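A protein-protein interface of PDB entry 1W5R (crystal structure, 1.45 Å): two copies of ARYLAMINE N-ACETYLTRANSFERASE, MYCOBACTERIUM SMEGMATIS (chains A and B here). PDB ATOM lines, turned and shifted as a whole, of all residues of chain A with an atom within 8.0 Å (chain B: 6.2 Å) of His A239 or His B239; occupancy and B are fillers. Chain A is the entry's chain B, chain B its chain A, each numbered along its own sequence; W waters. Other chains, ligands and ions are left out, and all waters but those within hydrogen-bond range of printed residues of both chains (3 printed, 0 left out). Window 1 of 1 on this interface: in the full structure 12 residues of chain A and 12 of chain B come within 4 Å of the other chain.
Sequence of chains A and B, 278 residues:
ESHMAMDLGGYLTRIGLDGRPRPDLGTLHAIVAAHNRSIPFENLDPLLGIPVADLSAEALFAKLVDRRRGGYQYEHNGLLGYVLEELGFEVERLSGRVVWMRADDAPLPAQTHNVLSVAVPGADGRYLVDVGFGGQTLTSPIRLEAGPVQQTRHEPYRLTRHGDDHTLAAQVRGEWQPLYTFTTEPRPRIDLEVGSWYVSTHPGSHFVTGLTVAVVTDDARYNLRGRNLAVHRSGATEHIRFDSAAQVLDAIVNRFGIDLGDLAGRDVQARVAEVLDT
His A239 touches two residues of chain B.
His B239 touches just these residues of chain A: Thr A237, Glu A238 and His A239.
Of the printed residues of chain A, Ile B240 touches Thr A237 and Glu A238.
Of the printed residues of chain A, Arg B241 touches Ala A236 and Thr A237.
Printed residues of chain B within 4 Å of Ala A236: Arg B241 (3.4 Å).
Asn A228 touches none of the printed residues of chain B.
The nearest residue of chain B that does not touch His A239 is Thr B237 (4.1 Å).
The nearest residue of chain A that does not touch His B239 is Ile A240 (4.8 Å).
Thr A237 touches Ile B240, and with the chains exchanged Ile A240 touches Thr B237.
Thr A237 touches Arg B241, and with the chains exchanged Arg A241 touches Thr B237.
Glu A238 touches Ile B240, and with the chains exchanged Ile A240 touches Glu B238.
His A239 touches its own counterpart, His B239.
The backbone carbonyl oxygen (O) of Thr B237 sits at hydrogen-bond distance from the backbone NH (N) of Arg A241 (2.9 Å).
N of His B239 is in hydrogen-bond range of O of His A239 (2.8 Å).
The backbone NH (N) of Arg B241 sits at hydrogen-bond distance from the backbone carbonyl oxygen (O) of Thr A237.
Among the printed residues, merely in contact across the chains: Glu A238 with His B239 (3.3 Å), Ile A240 with Thr B237 (3.3 Å), Ala A236 with Arg B241 (3.4 Å), Thr A237 with Ile B240 (3.5 Å), His A239 with Glu B238 (3.5 Å), Ile A240 with Glu B238 (3.8 Å), Glu A238 with Ile B240 (3.9 Å) and Thr A237 with His B239 (3.9 Å).
Of the 9 printed residues of chain B, 5 touch a printed residue of chain A.
Printed residues of chain B that touch a printed residue of chain A: Thr B237, Glu B238, His B239, Ile B240 and Arg B241.
Hydrophobic or aromatic side chains of chain A that line the printed part of chain B: Ala A236 and Ile A240.
Among the printed residues, no Asp or Glu carboxylate lies within 4 Å of a Lys or Arg side-chain nitrogen of the other chain.
N of Leu B229 is in hydrogen-bond range of O of Ile B240.
The backbone carbonyl oxygen of Val B231 sits at hydrogen-bond distance from the backbone NH of Glu B238 (2.8 Å).
N of Ile A240 is in hydrogen-bond range of O of Leu A229.
The backbone carbonyl oxygen (O) of Val A231 is in hydrogen-bond range of the backbone NH (N) of Glu A238 (2.8 Å).
Water W2 lies within hydrogen-bond range of OE1 of Glu B238 (2.6 Å) and OE1 of Glu A238 (2.7 Å).
Water W3 lies within hydrogen-bond range of the backbone carbonyl oxygen (O) of His A239, the backbone carbonyl oxygen (O) of Thr B237 and a ring nitrogen (NE2) of His B239.
Water W1 bridges OG1 of Thr A237 (3.0 Å) and O of His B239 (3.1 Å).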
ATOM      1  N   ASN A 223      24.593  21.090  28.126  1.00  0.00           N
ATOM      2  CA  ASN A 223      25.789  20.326  27.817  1.00  0.00           C
ATOM      3  C   ASN A 223      26.790  21.157  27.050  1.00  0.00           C
ATOM      4  O   ASN A 223      26.504  21.588  25.929  1.00  0.00           O
ATOM      5  CB  ASN A 223      25.445  19.076  27.017  1.00  0.00           C
ATOM      6  CG  ASN A 223      26.666  18.191  26.792  1.00  0.00           C
ATOM      7  OD1 ASN A 223      27.349  17.811  27.744  1.00  0.00           O
ATOM      8  ND2 ASN A 223      26.960  17.894  25.537  1.00  0.00           N
ATOM      9  N   ARG A 225      30.501  21.378  25.303  1.00  0.00           N
ATOM     10  CA  ARG A 225      31.706  20.758  24.765  1.00  0.00           C
ATOM     11  C   ARG A 225      32.590  21.870  24.224  1.00  0.00           C
ATOM     12  O   ARG A 225      32.191  22.568  23.296  1.00  0.00           O
ATOM     13  CB  ARG A 225      31.382  19.746  23.655  1.00  0.00           C
ATOM     14  CG  ARG A 225      32.621  19.140  22.982  1.00  0.00           C
ATOM     15  CD  ARG A 225      33.330  18.170  23.925  1.00  0.00           C
ATOM     16  NE  ARG A 225      34.524  17.596  23.314  1.00  0.00           N
ATOM     17  CZ  ARG A 225      35.287  16.675  23.904  1.00  0.00           C
ATOM     18  NH1 ARG A 225      34.977  16.243  25.117  1.00  0.00           N
ATOM     19  NH2 ARG A 225      36.350  16.191  23.275  1.00  0.00           N
ATOM     20  N   ARG A 227      33.892  25.242  23.451  1.00  0.00           N
ATOM     21  CA  ARG A 227      33.256  26.570  23.476  1.00  0.00           C
ATOM     22  C   ARG A 227      31.738  26.539  23.285  1.00  0.00           C
ATOM     23  O   ARG A 227      31.070  27.591  23.344  1.00  0.00           O
ATOM     24  CB  ARG A 227      33.868  27.481  22.399  1.00  0.00           C
ATOM     25  CG  ARG A 227      33.515  27.025  21.006  1.00  0.00           C
ATOM     26  CD  ARG A 227      33.916  28.026  19.947  1.00  0.00           C
ATOM     27  NE  ARG A 227      35.323  27.960  19.577  1.00  0.00           N
ATOM     28  CZ  ARG A 227      36.188  28.955  19.766  1.00  0.00           C
ATOM     29  NH1 ARG A 227      35.811  30.068  20.384  1.00  0.00           N
ATOM     30  NH2 ARG A 227      37.442  28.826  19.357  1.00  0.00           N
ATOM     31  N   ASN A 228      31.199  25.350  23.019  1.00  0.00           N
ATOM     32  CA  ASN A 228      29.814  25.198  22.553  1.00  0.00           C
ATOM     33  C   ASN A 228      28.895  24.639  23.627  1.00  0.00           C
ATOM     34  O   ASN A 228      29.037  23.484  24.046  1.00  0.00           O
ATOM     35  CB  ASN A 228      29.762  24.302  21.313  1.00  0.00           C
ATOM     36  CG  ASN A 228      30.590  24.857  20.167  1.00  0.00           C
ATOM     37  OD1 ASN A 228      30.304  25.931  19.655  1.00  0.00           O
ATOM     38  ND2 ASN A 228      31.631  24.131  19.776  1.00  0.00           N
ATOM     39  N   LEU A 229      27.977  25.472  24.093  1.00  0.00           N
ATOM     40  CA  LEU A 229      26.961  25.065  25.060  1.00  0.00           C
ATOM     41  C   LEU A 229      25.618  24.781  24.384  1.00  0.00           C
ATOM     42  O   LEU A 229      25.043  25.670  23.747  1.00  0.00           O
ATOM     43  CB  LEU A 229      26.797  26.144  26.137  1.00  0.00           C
ATOM     44  CG  LEU A 229      25.659  26.026  27.156  1.00  0.00           C
ATOM     45  CD1 LEU A 229      25.833  24.803  28.026  1.00  0.00           C
ATOM     46  CD2 LEU A 229      25.602  27.275  28.008  1.00  0.00           C
ATOM     47  N   ALA A 230      25.141  23.542  24.489  1.00  0.00           N
ATOM     48  CA  ALA A 230      23.808  23.162  24.012  1.00  0.00           C
ATOM     49  C   ALA A 230      22.832  23.123  25.173  1.00  0.00           C
ATOM     50  O   ALA A 230      23.170  22.684  26.277  1.00  0.00           O
ATOM     51  CB  ALA A 230      23.853  21.821  23.303  1.00  0.00           C
ATOM     52  N   VAL A 231      21.626  23.625  24.919  1.00  0.00           N
ATOM     53  CA  VAL A 231      20.555  23.634  25.904  1.00  0.00           C
ATOM     54  C   VAL A 231      19.336  22.996  25.249  1.00  0.00           C
ATOM     55  O   VAL A 231      18.941  23.384  24.154  1.00  0.00           O
ATOM     56  CB  VAL A 231      20.199  25.071  26.378  1.00  0.00           C
ATOM     57  CG1 VAL A 231      19.264  25.022  27.597  1.00  0.00           C
ATOM     58  CG2 VAL A 231      21.462  25.877  26.696  1.00  0.00           C
ATOM     59  N   HIS A 232      18.758  21.995  25.907  1.00  0.00           N
ATOM     60  CA  HIS A 232      17.479  21.439  25.463  1.00  0.00           C
ATOM     61  C   HIS A 232      16.447  21.825  26.500  1.00  0.00           C
ATOM     62  O   HIS A 232      16.607  21.541  27.685  1.00  0.00           O
ATOM     63  CB  HIS A 232      17.552  19.911  25.336  1.00  0.00           C
ATOM     64  CG  HIS A 232      18.272  19.439  24.114  1.00  0.00           C
ATOM     65  ND1 HIS A 232      18.237  18.124  23.693  1.00  0.00           N
ATOM     66  CD2 HIS A 232      19.036  20.103  23.212  1.00  0.00           C
ATOM     67  CE1 HIS A 232      18.961  17.997  22.595  1.00  0.00           C
ATOM     68  NE2 HIS A 232      19.449  19.186  22.277  1.00  0.00           N
ATOM     69  N   ALA A 236      12.236  24.400  22.503  1.00  0.00           N
ATOM     70  CA  ALA A 236      13.402  25.013  21.874  1.00  0.00           C
ATOM     71  C   ALA A 236      14.706  24.275  22.173  1.00  0.00           C
ATOM     72  O   ALA A 236      14.835  23.613  23.213  1.00  0.00           O
ATOM     73  CB  ALA A 236      13.514  26.474  22.300  1.00  0.00           C
ATOM     74  N   THR A 237      15.658  24.386  21.251  1.00  0.00           N
ATOM     75  CA  THR A 237      17.056  24.063  21.538  1.00  0.00           C
ATOM     76  C   THR A 237      17.843  25.368  21.460  1.00  0.00           C
ATOM     77  O   THR A 237      17.437  26.303  20.759  1.00  0.00           O
ATOM     78  CB  THR A 237      17.668  23.050  20.544  1.00  0.00           C
ATOM     79  OG1 THR A 237      17.670  23.590  19.221  1.00  0.00           O
ATOM     80  CG2 THR A 237      16.915  21.716  20.552  1.00  0.00           C
ATOM     81  N   GLU A 238      18.943  25.442  22.198  1.00  0.00           N
ATOM     82  CA  GLU A 238      19.840  26.586  22.111  1.00  0.00           C
ATOM     83  C   GLU A 238      21.253  26.102  21.880  1.00  0.00           C
ATOM     84  O   GLU A 238      21.644  25.053  22.386  1.00  0.00           O
ATOM     85  CB  GLU A 238      19.825  27.420  23.386  1.00  0.00           C
ATOM     86  CG  GLU A 238      18.461  27.717  23.950  1.00  0.00           C
ATOM     87  CD  GLU A 238      18.494  28.653  25.131  1.00  0.00           C
ATOM     88  OE1 GLU A 238      19.596  29.048  25.589  1.00  0.00           O
ATOM     89  OE2 GLU A 238      17.406  29.015  25.612  1.00  0.00           O
ATOM     90  N   HIS A 239      22.015  26.889  21.136  1.00  0.00           N
ATOM     91  CA  HIS A 239      23.447  26.694  20.979  1.00  0.00           C
ATOM     92  C   HIS A 239      24.130  28.018  21.285  1.00  0.00           C
ATOM     93  O   HIS A 239      23.946  28.997  20.554  1.00  0.00           O
ATOM     94  CB  HIS A 239      23.771  26.197  19.570  1.00  0.00           C
ATOM     95  CG  HIS A 239      25.217  26.315  19.186  1.00  0.00           C
ATOM     96  ND1 HIS A 239      26.252  26.165  20.088  1.00  0.00           N
ATOM     97  CD2 HIS A 239      25.798  26.550  17.983  1.00  0.00           C
ATOM     98  CE1 HIS A 239      27.405  26.316  19.459  1.00  0.00           C
ATOM     99  NE2 HIS A 239      27.158  26.543  18.181  1.00  0.00           N
ATOM    100  N   ILE A 240      24.878  28.052  22.382  1.00  0.00           N
ATOM    101  CA  ILE A 240      25.652  29.224  22.775  1.00  0.00           C
ATOM    102  C   ILE A 240      27.109  28.968  22.434  1.00  0.00           C
ATOM    103  O   ILE A 240      27.673  27.950  22.851  1.00  0.00           O
ATOM    104  CB  ILE A 240      25.486  29.546  24.269  1.00  0.00           C
ATOM    105  CG1 ILE A 240      24.014  29.867  24.578  1.00  0.00           C
ATOM    106  CG2 ILE A 240      26.416  30.688  24.680  1.00  0.00           C
ATOM    107  CD1 ILE A 240      23.690  30.132  26.042  1.00  0.00           C
ATOM    108  N   ARG A 241      27.704  29.880  21.663  1.00  0.00           N
ATOM    109  CA  ARG A 241      29.106  29.776  21.287  1.00  0.00           C
ATOM    110  C   ARG A 241      29.916  30.836  22.019  1.00  0.00           C
ATOM    111  O   ARG A 241      29.750  32.040  21.779  1.00  0.00           O
ATOM    112  CB  ARG A 241      29.289  29.906  19.778  1.00  0.00           C
ATOM    113  CG  ARG A 241      30.705  29.666  19.306  1.00  0.00           C
ATOM    114  CD  ARG A 241      30.890  30.166  17.876  1.00  0.00           C
ATOM    115  NE  ARG A 241      32.198  29.832  17.313  1.00  0.00           N
ATOM    116  CZ  ARG A 241      33.302  30.562  17.465  1.00  0.00           C
ATOM    117  NH1 ARG A 241      33.288  31.674  18.194  1.00  0.00           N
ATOM    118  NH2 ARG A 241      34.438  30.164  16.894  1.00  0.00           N
ATOM    119  N   PHE A 242      30.795  30.392  22.908  1.00  0.00           N
ATOM    120  CA  PHE A 242      31.673  31.300  23.639  1.00  0.00           C
ATOM    121  C   PHE A 242      32.856  31.764  22.797  1.00  0.00           C
ATOM    122  O   PHE A 242      33.412  30.999  22.008  1.00  0.00           O
ATOM    123  CB  PHE A 242      32.144  30.661  24.940  1.00  0.00           C
ATOM    124  CG  PHE A 242      31.035  30.449  25.927  1.00  0.00           C
ATOM    125  CD1 PHE A 242      30.673  29.168  26.321  1.00  0.00           C
ATOM    126  CD2 PHE A 242      30.333  31.528  26.440  1.00  0.00           C
ATOM    127  CE1 PHE A 242      29.631  28.972  27.230  1.00  0.00           C
ATOM    128  CE2 PHE A 242      29.295  31.336  27.329  1.00  0.00           C
ATOM    129  CZ  PHE A 242      28.945  30.048  27.732  1.00  0.00           C
ATOM    130  N   LEU B 229      16.309  32.378  16.400  1.00  0.00           N
ATOM    131  CA  LEU B 229      16.606  33.594  17.132  1.00  0.00           C
ATOM    132  C   LEU B 229      18.098  33.686  17.408  1.00  0.00           C
ATOM    133  O   LEU B 229      18.659  32.864  18.147  1.00  0.00           O
ATOM    134  CB  LEU B 229      15.804  33.644  18.429  1.00  0.00           C
ATOM    135  CG  LEU B 229      16.119  34.750  19.430  1.00  0.00           C
ATOM    136  CD1 LEU B 229      15.911  36.128  18.788  1.00  0.00           C
ATOM    137  CD2 LEU B 229      15.250  34.620  20.669  1.00  0.00           C
ATOM    138  N   ALA B 230      18.754  34.671  16.804  1.00  0.00           N
ATOM    139  CA  ALA B 230      20.166  34.938  17.098  1.00  0.00           C
ATOM    140  C   ALA B 230      20.299  36.027  18.162  1.00  0.00           C
ATOM    141  O   ALA B 230      19.587  37.045  18.122  1.00  0.00           O
ATOM    142  CB  ALA B 230      20.907  35.359  15.833  1.00  0.00           C
ATOM    143  N   VAL B 231      21.219  35.821  19.097  1.00  0.00           N
ATOM    144  CA  VAL B 231      21.527  36.815  20.113  1.00  0.00           C
ATOM    145  C   VAL B 231      23.036  37.064  20.071  1.00  0.00           C
ATOM    146  O   VAL B 231      23.830  36.131  20.164  1.00  0.00           O
ATOM    147  CB  VAL B 231      21.110  36.341  21.534  1.00  0.00           C
ATOM    148  CG1 VAL B 231      21.325  37.468  22.539  1.00  0.00           C
ATOM    149  CG2 VAL B 231      19.654  35.855  21.559  1.00  0.00           C
ATOM    150  N   HIS B 232      23.431  38.319  19.908  1.00  0.00           N
ATOM    151  CA  HIS B 232      24.830  38.702  20.000  1.00  0.00           C
ATOM    152  C   HIS B 232      25.032  39.510  21.273  1.00  0.00           C
ATOM    153  O   HIS B 232      24.414  40.562  21.462  1.00  0.00           O
ATOM    154  CB  HIS B 232      25.254  39.526  18.772  1.00  0.00           C
ATOM    155  CG  HIS B 232      25.498  38.702  17.546  1.00  0.00           C
ATOM    156  ND1 HIS B 232      26.093  39.212  16.411  1.00  0.00           N
ATOM    157  CD2 HIS B 232      25.218  37.407  17.272  1.00  0.00           C
ATOM    158  CE1 HIS B 232      26.178  38.264  15.495  1.00  0.00           C
ATOM    159  NE2 HIS B 232      25.650  37.160  15.991  1.00  0.00           N
ATOM    160  N   THR B 237      27.763  34.323  21.265  1.00  0.00           N
ATOM    161  CA  THR B 237      26.599  34.342  20.397  1.00  0.00           C
ATOM    162  C   THR B 237      25.671  33.254  20.922  1.00  0.00           C
ATOM    163  O   THR B 237      26.143  32.278  21.516  1.00  0.00           O
ATOM    164  CB  THR B 237      27.008  34.046  18.947  1.00  0.00           C
ATOM    165  OG1 THR B 237      27.893  35.074  18.488  1.00  0.00           O
ATOM    166  CG2 THR B 237      25.810  33.985  18.020  1.00  0.00           C
ATOM    167  N   GLU B 238      24.366  33.446  20.745  1.00  0.00           N
ATOM    168  CA  GLU B 238      23.367  32.423  21.048  1.00  0.00           C
ATOM    169  C   GLU B 238      22.497  32.191  19.832  1.00  0.00           C
ATOM    170  O   GLU B 238      22.135  33.139  19.127  1.00  0.00           O
ATOM    171  CB  GLU B 238      22.474  32.846  22.211  1.00  0.00           C
ATOM    172  CG  GLU B 238      23.211  33.388  23.416  1.00  0.00           C
ATOM    173  CD  GLU B 238      22.283  33.843  24.527  1.00  0.00           C
ATOM    174  OE1 GLU B 238      21.049  33.620  24.438  1.00  0.00           O
ATOM    175  OE2 GLU B 238      22.798  34.423  25.504  1.00  0.00           O
ATOM    176  N   HIS B 239      22.174  30.931  19.581  1.00  0.00           N
ATOM    177  CA  HIS B 239      21.230  30.570  18.548  1.00  0.00           C
ATOM    178  C   HIS B 239      20.127  29.732  19.161  1.00  0.00           C
ATOM    179  O   HIS B 239      20.368  28.605  19.593  1.00  0.00           O
ATOM    180  CB  HIS B 239      21.929  29.857  17.387  1.00  0.00           C
ATOM    181  CG  HIS B 239      22.903  30.731  16.655  1.00  0.00           C
ATOM    182  ND1 HIS B 239      22.537  31.925  16.071  1.00  0.00           N
ATOM    183  CD2 HIS B 239      24.232  30.594  16.424  1.00  0.00           C
ATOM    184  CE1 HIS B 239      23.595  32.485  15.512  1.00  0.00           C
ATOM    185  NE2 HIS B 239      24.638  31.697  15.712  1.00  0.00           N
ATOM    186  N   ILE B 240      18.933  30.305  19.234  1.00  0.00           N
ATOM    187  CA  ILE B 240      17.769  29.628  19.776  1.00  0.00           C
ATOM    188  C   ILE B 240      16.914  29.152  18.605  1.00  0.00           C
ATOM    189  O   ILE B 240      16.466  29.956  17.766  1.00  0.00           O
ATOM    190  CB  ILE B 240      16.986  30.558  20.744  1.00  0.00           C
ATOM    191  CG1 ILE B 240      17.886  30.971  21.916  1.00  0.00           C
ATOM    192  CG2 ILE B 240      15.701  29.896  21.225  1.00  0.00           C
ATOM    193  CD1 ILE B 240      17.471  32.241  22.624  1.00  0.00           C
ATOM    194  N   ARG B 241      16.700  27.842  18.526  1.00  0.00           N
ATOM    195  CA  ARG B 241      15.896  27.265  17.447  1.00  0.00           C
ATOM    196  C   ARG B 241      14.557  26.798  18.003  1.00  0.00           C
ATOM    197  O   ARG B 241      14.483  25.829  18.765  1.00  0.00           O
ATOM    198  CB  ARG B 241      16.644  26.108  16.771  1.00  0.00           C
ATOM    199  CG  ARG B 241      15.912  25.491  15.584  1.00  0.00           C
ATOM    200  CD  ARG B 241      16.588  24.201  15.101  1.00  0.00           C
ATOM    201  NE  ARG B 241      15.900  23.634  13.940  1.00  0.00           N
ATOM    202  CZ  ARG B 241      14.787  22.894  13.998  1.00  0.00           C
ATOM    203  NH1 ARG B 241      14.194  22.629  15.156  1.00  0.00           N
ATOM    204  NH2 ARG B 241      14.257  22.432  12.877  1.00  0.00           N
HETATM  205  O   HOH W   1      19.807  25.637  18.707  1.00  0.00           O
HETATM  206  O   HOH W   2      20.141  31.669  25.940  1.00  0.00           O
HETATM  207  O   HOH W   3      25.620  30.533  18.848  1.00  0.00           O
